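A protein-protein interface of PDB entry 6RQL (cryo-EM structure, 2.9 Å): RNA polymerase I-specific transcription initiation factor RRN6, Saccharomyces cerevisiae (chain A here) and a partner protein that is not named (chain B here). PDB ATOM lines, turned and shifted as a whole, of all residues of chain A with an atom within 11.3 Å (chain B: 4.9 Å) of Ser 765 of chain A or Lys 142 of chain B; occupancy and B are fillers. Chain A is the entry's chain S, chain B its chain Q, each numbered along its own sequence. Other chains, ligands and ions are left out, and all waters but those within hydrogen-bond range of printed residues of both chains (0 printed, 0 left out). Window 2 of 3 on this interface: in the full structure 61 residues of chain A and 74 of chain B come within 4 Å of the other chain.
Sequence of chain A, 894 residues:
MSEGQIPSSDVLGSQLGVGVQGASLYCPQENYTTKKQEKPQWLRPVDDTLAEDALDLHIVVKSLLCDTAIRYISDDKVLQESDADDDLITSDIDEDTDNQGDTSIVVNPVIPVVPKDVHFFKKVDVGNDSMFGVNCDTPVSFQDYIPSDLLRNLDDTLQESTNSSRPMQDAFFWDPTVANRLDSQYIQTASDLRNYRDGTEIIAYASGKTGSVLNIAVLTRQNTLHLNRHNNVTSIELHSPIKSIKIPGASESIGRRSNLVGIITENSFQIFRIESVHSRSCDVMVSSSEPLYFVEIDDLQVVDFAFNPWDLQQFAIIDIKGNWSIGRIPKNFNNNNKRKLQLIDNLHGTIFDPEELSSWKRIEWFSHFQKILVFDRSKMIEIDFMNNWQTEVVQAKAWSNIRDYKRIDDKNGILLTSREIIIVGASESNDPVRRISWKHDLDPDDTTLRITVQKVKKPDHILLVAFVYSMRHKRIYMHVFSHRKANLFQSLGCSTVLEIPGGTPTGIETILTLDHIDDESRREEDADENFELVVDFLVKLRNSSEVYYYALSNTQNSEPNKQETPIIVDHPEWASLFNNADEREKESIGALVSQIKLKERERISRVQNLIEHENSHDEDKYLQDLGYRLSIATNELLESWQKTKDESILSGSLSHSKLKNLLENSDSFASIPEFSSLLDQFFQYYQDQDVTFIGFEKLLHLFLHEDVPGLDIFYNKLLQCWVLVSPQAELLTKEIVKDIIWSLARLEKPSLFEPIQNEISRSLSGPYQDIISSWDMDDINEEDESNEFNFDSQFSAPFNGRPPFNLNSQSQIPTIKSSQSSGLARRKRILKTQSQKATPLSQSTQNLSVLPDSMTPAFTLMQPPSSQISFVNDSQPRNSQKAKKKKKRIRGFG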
ATOM      1  N   SER A 648      19.873  21.133  -9.458  1.00  0.00           N
ATOM      2  CA  SER A 648      19.365  20.171  -8.476  1.00  0.00           C
ATOM      3  C   SER A 648      19.573  18.733  -8.951  1.00  0.00           C
ATOM      4  O   SER A 648      18.634  17.967  -9.167  1.00  0.00           O
ATOM      5  CB  SER A 648      17.897  20.449  -8.136  1.00  0.00           C
ATOM      6  OG  SER A 648      17.763  21.704  -7.493  1.00  0.00           O
ATOM      7  N   ILE A 649      20.844  18.393  -9.131  1.00  0.00           N
ATOM      8  CA  ILE A 649      21.244  17.080  -9.605  1.00  0.00           C
ATOM      9  C   ILE A 649      22.281  16.488  -8.657  1.00  0.00           C
ATOM     10  O   ILE A 649      22.796  17.181  -7.776  1.00  0.00           O
ATOM     11  CB  ILE A 649      21.786  17.156 -11.041  1.00  0.00           C
ATOM     12  CG1 ILE A 649      21.986  15.756 -11.623  1.00  0.00           C
ATOM     13  CG2 ILE A 649      23.081  17.955 -11.075  1.00  0.00           C
ATOM     14  CD1 ILE A 649      20.707  14.995 -11.835  1.00  0.00           C
ATOM     15  N   GLN A 757      17.883  23.919  -1.118  1.00  0.00           N
ATOM     16  CA  GLN A 757      17.053  23.631  -2.281  1.00  0.00           C
ATOM     17  C   GLN A 757      17.404  22.284  -2.896  1.00  0.00           C
ATOM     18  O   GLN A 757      16.640  21.773  -3.723  1.00  0.00           O
ATOM     19  CB  GLN A 757      17.174  24.711  -3.361  1.00  0.00           C
ATOM     20  CG  GLN A 757      18.419  24.600  -4.224  1.00  0.00           C
ATOM     21  CD  GLN A 757      18.487  25.661  -5.297  1.00  0.00           C
ATOM     22  OE1 GLN A 757      17.567  26.463  -5.455  1.00  0.00           O
ATOM     23  NE2 GLN A 757      19.582  25.669  -6.050  1.00  0.00           N
ATOM     24  N   ASN A 758      18.548  21.709  -2.526  1.00  0.00           N
ATOM     25  CA  ASN A 758      18.933  20.390  -3.000  1.00  0.00           C
ATOM     26  C   ASN A 758      18.407  19.289  -2.094  1.00  0.00           C
ATOM     27  O   ASN A 758      17.952  18.255  -2.594  1.00  0.00           O
ATOM     28  CB  ASN A 758      20.457  20.297  -3.103  1.00  0.00           C
ATOM     29  CG  ASN A 758      20.922  19.125  -3.938  1.00  0.00           C
ATOM     30  OD1 ASN A 758      20.122  18.370  -4.486  1.00  0.00           O
ATOM     31  ND2 ASN A 758      22.230  18.966  -4.039  1.00  0.00           N
ATOM     32  N   GLU A 759      18.446  19.495  -0.774  1.00  0.00           N
ATOM     33  CA  GLU A 759      17.900  18.515   0.157  1.00  0.00           C
ATOM     34  C   GLU A 759      16.392  18.371   0.037  1.00  0.00           C
ATOM     35  O   GLU A 759      15.863  17.291   0.320  1.00  0.00           O
ATOM     36  CB  GLU A 759      18.256  18.883   1.596  1.00  0.00           C
ATOM     37  CG  GLU A 759      19.718  18.702   1.931  1.00  0.00           C
ATOM     38  CD  GLU A 759      20.063  19.124   3.347  1.00  0.00           C
ATOM     39  OE1 GLU A 759      19.174  19.638   4.054  1.00  0.00           O
ATOM     40  OE2 GLU A 759      21.227  18.941   3.756  1.00  0.00           O
ATOM     41  N   ILE A 760      15.691  19.416  -0.390  1.00  0.00           N
ATOM     42  CA  ILE A 760      14.268  19.272  -0.645  1.00  0.00           C
ATOM     43  C   ILE A 760      14.100  18.575  -1.986  1.00  0.00           C
ATOM     44  O   ILE A 760      13.130  17.838  -2.182  1.00  0.00           O
ATOM     45  CB  ILE A 760      13.530  20.624  -0.598  1.00  0.00           C
ATOM     46  CG1 ILE A 760      14.081  21.591  -1.644  1.00  0.00           C
ATOM     47  CG2 ILE A 760      13.626  21.231   0.789  1.00  0.00           C
ATOM     48  CD1 ILE A 760      13.270  22.845  -1.832  1.00  0.00           C
ATOM     49  N   SER A 761      15.068  18.751  -2.896  1.00  0.00           N
ATOM     50  CA  SER A 761      14.949  18.202  -4.242  1.00  0.00           C
ATOM     51  C   SER A 761      15.093  16.692  -4.263  1.00  0.00           C
ATOM     52  O   SER A 761      14.434  16.027  -5.071  1.00  0.00           O
ATOM     53  CB  SER A 761      16.000  18.821  -5.166  1.00  0.00           C
ATOM     54  OG  SER A 761      15.821  20.220  -5.282  1.00  0.00           O
ATOM     55  N   ARG A 762      15.930  16.143  -3.387  1.00  0.00           N
ATOM     56  CA  ARG A 762      16.087  14.701  -3.313  1.00  0.00           C
ATOM     57  C   ARG A 762      14.988  14.075  -2.459  1.00  0.00           C
ATOM     58  O   ARG A 762      14.645  12.902  -2.652  1.00  0.00           O
ATOM     59  CB  ARG A 762      17.481  14.379  -2.775  1.00  0.00           C
ATOM     60  CG  ARG A 762      17.859  12.912  -2.804  1.00  0.00           C
ATOM     61  CD  ARG A 762      17.979  12.396  -4.227  1.00  0.00           C
ATOM     62  NE  ARG A 762      19.106  12.991  -4.936  1.00  0.00           N
ATOM     63  CZ  ARG A 762      19.329  12.841  -6.236  1.00  0.00           C
ATOM     64  NH1 ARG A 762      20.379  13.421  -6.803  1.00  0.00           N
ATOM     65  NH2 ARG A 762      18.503  12.107  -6.972  1.00  0.00           N
ATOM     66  N   SER A 763      14.401  14.855  -1.545  1.00  0.00           N
ATOM     67  CA  SER A 763      13.277  14.385  -0.741  1.00  0.00           C
ATOM     68  C   SER A 763      12.014  14.143  -1.554  1.00  0.00           C
ATOM     69  O   SER A 763      11.150  13.375  -1.118  1.00  0.00           O
ATOM     70  CB  SER A 763      12.952  15.387   0.364  1.00  0.00           C
ATOM     71  OG  SER A 763      11.770  15.001   1.043  1.00  0.00           O
ATOM     72  N   LEU A 764      11.885  14.782  -2.714  1.00  0.00           N
ATOM     73  CA  LEU A 764      10.690  14.633  -3.525  1.00  0.00           C
ATOM     74  C   LEU A 764      10.691  13.357  -4.352  1.00  0.00           C
ATOM     75  O   LEU A 764       9.621  12.774  -4.551  1.00  0.00           O
ATOM     76  CB  LEU A 764      10.538  15.841  -4.452  1.00  0.00           C
ATOM     77  CG  LEU A 764      10.386  17.193  -3.758  1.00  0.00           C
ATOM     78  CD1 LEU A 764      10.337  18.322  -4.770  1.00  0.00           C
ATOM     79  CD2 LEU A 764       9.184  17.229  -2.829  1.00  0.00           C
ATOM     80  N   SER A 765      11.859  12.908  -4.821  1.00  0.00           N
ATOM     81  CA  SER A 765      11.929  11.731  -5.681  1.00  0.00           C
ATOM     82  C   SER A 765      11.667  10.439  -4.925  1.00  0.00           C
ATOM     83  O   SER A 765      11.314   9.433  -5.547  1.00  0.00           O
ATOM     84  CB  SER A 765      13.292  11.657  -6.366  1.00  0.00           C
ATOM     85  OG  SER A 765      13.387  10.488  -7.159  1.00  0.00           O
ATOM     86  N   GLY A 766      11.847  10.438  -3.609  1.00  0.00           N
ATOM     87  CA  GLY A 766      11.400   9.342  -2.790  1.00  0.00           C
ATOM     88  C   GLY A 766       9.923   9.482  -2.485  1.00  0.00           C
ATOM     89  O   GLY A 766       9.394  10.593  -2.387  1.00  0.00           O
ATOM     90  N   PRO A 767       9.232   8.366  -2.312  1.00  0.00           N
ATOM     91  CA  PRO A 767       7.791   8.409  -2.066  1.00  0.00           C
ATOM     92  C   PRO A 767       7.492   8.829  -0.632  1.00  0.00           C
ATOM     93  O   PRO A 767       8.373   9.180   0.147  1.00  0.00           O
ATOM     94  CB  PRO A 767       7.355   6.964  -2.320  1.00  0.00           C
ATOM     95  CG  PRO A 767       8.537   6.161  -1.961  1.00  0.00           C
ATOM     96  CD  PRO A 767       9.730   6.980  -2.362  1.00  0.00           C
ATOM     97  N   TYR A 768       6.202   8.758  -0.294  1.00  0.00           N
ATOM     98  CA  TYR A 768       5.681   8.919   1.060  1.00  0.00           C
ATOM     99  C   TYR A 768       6.267   7.926   2.049  1.00  0.00           C
ATOM    100  O   TYR A 768       6.220   8.180   3.256  1.00  0.00           O
ATOM    101  CB  TYR A 768       4.157   8.755   1.043  1.00  0.00           C
ATOM    102  CG  TYR A 768       3.667   7.389   0.574  1.00  0.00           C
ATOM    103  CD1 TYR A 768       3.450   7.136  -0.777  1.00  0.00           C
ATOM    104  CD2 TYR A 768       3.382   6.368   1.482  1.00  0.00           C
ATOM    105  CE1 TYR A 768       2.995   5.905  -1.209  1.00  0.00           C
ATOM    106  CE2 TYR A 768       2.929   5.136   1.057  1.00  0.00           C
ATOM    107  CZ  TYR A 768       2.734   4.911  -0.289  1.00  0.00           C
ATOM    108  OH  TYR A 768       2.275   3.688  -0.721  1.00  0.00           O
ATOM    109  N   GLN A 769       6.756   6.788   1.557  1.00  0.00           N
ATOM    110  CA  GLN A 769       7.310   5.755   2.415  1.00  0.00           C
ATOM    111  C   GLN A 769       8.577   6.249   3.098  1.00  0.00           C
ATOM    112  O   GLN A 769       8.770   6.032   4.297  1.00  0.00           O
ATOM    113  CB  GLN A 769       7.597   4.517   1.574  1.00  0.00           C
ATOM    114  CG  GLN A 769       7.595   3.257   2.357  1.00  0.00           C
ATOM    115  CD  GLN A 769       6.198   2.914   2.801  1.00  0.00           C
ATOM    116  OE1 GLN A 769       5.846   3.093   3.970  1.00  0.00           O
ATOM    117  NE2 GLN A 769       5.386   2.432   1.879  1.00  0.00           N
ATOM    118  N   ASP A 770       9.412   6.979   2.365  1.00  0.00           N
ATOM    119  CA  ASP A 770      10.704   7.424   2.859  1.00  0.00           C
ATOM    120  C   ASP A 770      10.675   8.865   3.362  1.00  0.00           C
ATOM    121  O   ASP A 770      11.711   9.365   3.808  1.00  0.00           O
ATOM    122  CB  ASP A 770      11.752   7.275   1.755  1.00  0.00           C
ATOM    123  CG  ASP A 770      11.871   5.842   1.244  1.00  0.00           C
ATOM    124  OD1 ASP A 770      11.604   4.900   2.015  1.00  0.00           O
ATOM    125  OD2 ASP A 770      12.221   5.659   0.061  1.00  0.00           O
ATOM    126  N   ILE A 771       9.520   9.543   3.291  1.00  0.00           N
ATOM    127  CA  ILE A 771       9.405  10.915   3.793  1.00  0.00           C
ATOM    128  C   ILE A 771       9.572  10.952   5.307  1.00  0.00           C
ATOM    129  O   ILE A 771      10.420  11.681   5.834  1.00  0.00           O
ATOM    130  CB  ILE A 771       8.061  11.547   3.370  1.00  0.00           C
ATOM    131  CG1 ILE A 771       8.035  11.883   1.878  1.00  0.00           C
ATOM    132  CG2 ILE A 771       7.761  12.815   4.173  1.00  0.00           C
ATOM    133  CD1 ILE A 771       9.025  12.963   1.473  1.00  0.00           C
ATOM    134  N   SER A 773      10.653   8.561   7.135  1.00  0.00           N
ATOM    135  CA  SER A 773      11.969   7.987   7.382  1.00  0.00           C
ATOM    136  C   SER A 773      13.111   8.946   7.073  1.00  0.00           C
ATOM    137  O   SER A 773      14.263   8.595   7.330  1.00  0.00           O
ATOM    138  CB  SER A 773      12.140   6.713   6.558  1.00  0.00           C
ATOM    139  OG  SER A 773      13.444   6.185   6.701  1.00  0.00           O
ATOM    140  N   SER A 774      12.834  10.126   6.526  1.00  0.00           N
ATOM    141  CA  SER A 774      13.835  11.164   6.291  1.00  0.00           C
ATOM    142  C   SER A 774      13.508  12.302   7.243  1.00  0.00           C
ATOM    143  O   SER A 774      12.861  13.278   6.863  1.00  0.00           O
ATOM    144  CB  SER A 774      13.828  11.639   4.853  1.00  0.00           C
ATOM    145  OG  SER A 774      14.691  12.749   4.694  1.00  0.00           O
ATOM    146  N   LEU B 138      20.727  11.352   1.804  1.00  0.00           N
ATOM    147  CA  LEU B 138      19.521  11.363   0.980  1.00  0.00           C
ATOM    148  C   LEU B 138      19.751  10.727  -0.381  1.00  0.00           C
ATOM    149  O   LEU B 138      18.805  10.202  -0.980  1.00  0.00           O
ATOM    150  CB  LEU B 138      18.979  12.781   0.813  1.00  0.00           C
ATOM    151  CG  LEU B 138      18.268  13.313   2.059  1.00  0.00           C
ATOM    152  CD1 LEU B 138      17.878  14.779   1.915  1.00  0.00           C
ATOM    153  CD2 LEU B 138      17.070  12.445   2.368  1.00  0.00           C
ATOM    154  N   LYS B 139      20.981  10.751  -0.887  1.00  0.00           N
ATOM    155  CA  LYS B 139      21.238  10.083  -2.153  1.00  0.00           C
ATOM    156  C   LYS B 139      21.327   8.572  -2.016  1.00  0.00           C
ATOM    157  O   LYS B 139      21.050   7.859  -2.987  1.00  0.00           O
ATOM    158  CB  LYS B 139      22.510  10.620  -2.810  1.00  0.00           C
ATOM    159  CG  LYS B 139      22.338  12.023  -3.357  1.00  0.00           C
ATOM    160  CD  LYS B 139      23.395  12.355  -4.390  1.00  0.00           C
ATOM    161  CE  LYS B 139      24.743  12.585  -3.777  1.00  0.00           C
ATOM    162  NZ  LYS B 139      25.691  12.971  -4.840  1.00  0.00           N
ATOM    163  N   ILE B 140      21.704   8.064  -0.843  1.00  0.00           N
ATOM    164  CA  ILE B 140      21.620   6.625  -0.615  1.00  0.00           C
ATOM    165  C   ILE B 140      20.229   6.225  -0.150  1.00  0.00           C
ATOM    166  O   ILE B 140      19.838   5.064  -0.313  1.00  0.00           O
ATOM    167  CB  ILE B 140      22.754   6.210   0.349  1.00  0.00           C
ATOM    168  CG1 ILE B 140      23.013   4.701   0.300  1.00  0.00           C
ATOM    169  CG2 ILE B 140      22.463   6.638   1.771  1.00  0.00           C
ATOM    170  CD1 ILE B 140      23.568   4.221  -1.009  1.00  0.00           C
ATOM    171  N   LEU B 141      19.442   7.165   0.369  1.00  0.00           N
ATOM    172  CA  LEU B 141      18.050   6.893   0.702  1.00  0.00           C
ATOM    173  C   LEU B 141      17.160   6.897  -0.534  1.00  0.00           C
ATOM    174  O   LEU B 141      16.155   6.177  -0.572  1.00  0.00           O
ATOM    175  CB  LEU B 141      17.550   7.923   1.719  1.00  0.00           C
ATOM    176  CG  LEU B 141      16.211   7.780   2.432  1.00  0.00           C
ATOM    177  CD1 LEU B 141      16.194   6.521   3.262  1.00  0.00           C
ATOM    178  CD2 LEU B 141      16.001   8.985   3.321  1.00  0.00           C
ATOM    179  N   LYS B 142      17.517   7.693  -1.546  1.00  0.00           N
ATOM    180  CA  LYS B 142      16.912   7.570  -2.867  1.00  0.00           C
ATOM    181  C   LYS B 142      17.350   6.290  -3.573  1.00  0.00           C
ATOM    182  O   LYS B 142      16.623   5.790  -4.438  1.00  0.00           O
ATOM    183  CB  LYS B 142      17.263   8.812  -3.698  1.00  0.00           C
ATOM    184  CG  LYS B 142      16.584   8.941  -5.066  1.00  0.00           C
ATOM    185  CD  LYS B 142      17.512   8.503  -6.202  1.00  0.00           C
ATOM    186  CE  LYS B 142      16.863   8.665  -7.561  1.00  0.00           C
ATOM    187  NZ  LYS B 142      15.736   7.709  -7.726  1.00  0.00           N
ATOM    188  N   THR B 143      18.520   5.752  -3.226  1.00  0.00           N
ATOM    189  CA  THR B 143      18.983   4.520  -3.852  1.00  0.00           C
ATOM    190  C   THR B 143      18.131   3.335  -3.416  1.00  0.00           C
ATOM    191  O   THR B 143      17.830   2.445  -4.221  1.00  0.00           O
ATOM    192  CB  THR B 143      20.457   4.303  -3.511  1.00  0.00           C
ATOM    193  OG1 THR B 143      21.207   5.452  -3.923  1.00  0.00           O
ATOM    194  CG2 THR B 143      21.014   3.079  -4.220  1.00  0.00           C
ATOM    195  N   ILE B 144      17.684   3.342  -2.158  1.00  0.00           N
ATOM    196  CA  ILE B 144      16.823   2.283  -1.639  1.00  0.00           C
ATOM    197  C   ILE B 144      15.448   2.331  -2.301  1.00  0.00           C
ATOM    198  O   ILE B 144      14.785   1.295  -2.453  1.00  0.00           O
ATOM    199  CB  ILE B 144      16.750   2.415  -0.104  1.00  0.00           C
ATOM    200  CG1 ILE B 144      18.162   2.386   0.482  1.00  0.00           C
ATOM    201  CG2 ILE B 144      15.914   1.320   0.542  1.00  0.00           C
ATOM    202  CD1 ILE B 144      18.951   1.145   0.132  1.00  0.00           C
ATOM    203  N   ASN B 145      15.020   3.523  -2.733  1.00  0.00           N
ATOM    204  CA  ASN B 145      13.752   3.690  -3.442  1.00  0.00           C
ATOM    205  C   ASN B 145      13.732   2.908  -4.751  1.00  0.00           C
ATOM    206  O   ASN B 145      12.729   2.271  -5.091  1.00  0.00           O
ATOM    207  CB  ASN B 145      13.525   5.174  -3.722  1.00  0.00           C
ATOM    208  CG  ASN B 145      12.165   5.468  -4.321  1.00  0.00           C
ATOM    209  OD1 ASN B 145      11.269   4.625  -4.348  1.00  0.00           O
ATOM    210  ND2 ASN B 145      12.018   6.676  -4.848  1.00  0.00           N
ATOM    211  N   ASP B 146      14.839   2.934  -5.493  1.00  0.00           N
ATOM    212  CA  ASP B 146      14.793   2.533  -6.893  1.00  0.00           C
ATOM    213  C   ASP B 146      14.788   1.018  -7.068  1.00  0.00           C
ATOM    214  O   ASP B 146      14.540   0.533  -8.176  1.00  0.00           O
ATOM    215  CB  ASP B 146      15.966   3.178  -7.632  1.00  0.00           C
ATOM    216  CG  ASP B 146      15.758   3.227  -9.130  1.00  0.00           C
ATOM    217  OD1 ASP B 146      14.916   4.031  -9.580  1.00  0.00           O
ATOM    218  OD2 ASP B 146      16.443   2.478  -9.856  1.00  0.00           O
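O of Lys 139 of chain B is in hydrogen-bond range of OG1 of Thr 143 of chain B (2.6 Å).
Of the 19 printed residues of chain A, 6 touch a printed residue of chain B.
Hydrophobic or aromatic side chains of chain A within 4 Å of the printed part of chain B: Pro 767.
Printed residues of chain B that touch a printed residue of chain A: Leu 138, Lys 139, Leu 141, Lys 142 and Asn 145.
Hydrophobic or aromatic side chains of chain B within 4 Å of the printed part of chain A: Leu 138 and Leu 141.
ND2 of Asn 145 of chain B is in hydrogen-bond range of O of Ser 765 of chain A, 2.9 Å away.
Among the printed residues, merely in contact across the chains: Ser 774 of chain A with Leu 138 of chain B, Pro 767 of chain A with Asn 145 of chain B, Arg 762 of chain A with Leu 138 of chain B, Gly 766 of chain A with Asn 145 of chain B, Glu 759 of chain A with Leu 138 of chain B, Ser 765 of chain A with Lys 142 of chain B, Arg 762 of chain A with Lys 142 of chain B, Arg 762 of chain A with Lys 139 of chain B and Ser 774 of chain A with Leu 141 of chain B.
Of chain B, only Lys 142 (3.7 Å) and Asn 145 (2.9 Å) come within 4 Å of Ser 765 of chain A.
Of chain A, only Arg 762 (3.7 Å) and Ser 765 (3.7 Å) come within 4 Å of Lys 142 of chain B.
No residue of chain A comes within 4 Å of Ile 140 of chain B.
No residue of chain A comes within 4 Å of Ile 144 of chain B.
Of the printed residues of chain A, Asn 145 of chain B touches Ser 765, Gly 766 and Pro 767.
No residue of chain A comes within 4 Å of Asp 146 of chain B.
Of the printed residues of chain B, Gly 766 of chain A touches Asn 145.
Of the printed residues of chain B, Glu 759 of chain A touches Leu 138 (3.6 Å).
Ile 771 of chain A touches none of the printed residues of chain B.
The nearest printed residue of chain B that does not touch Ser 774 of chain A is Lys 142 of chain B (8.4 Å).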
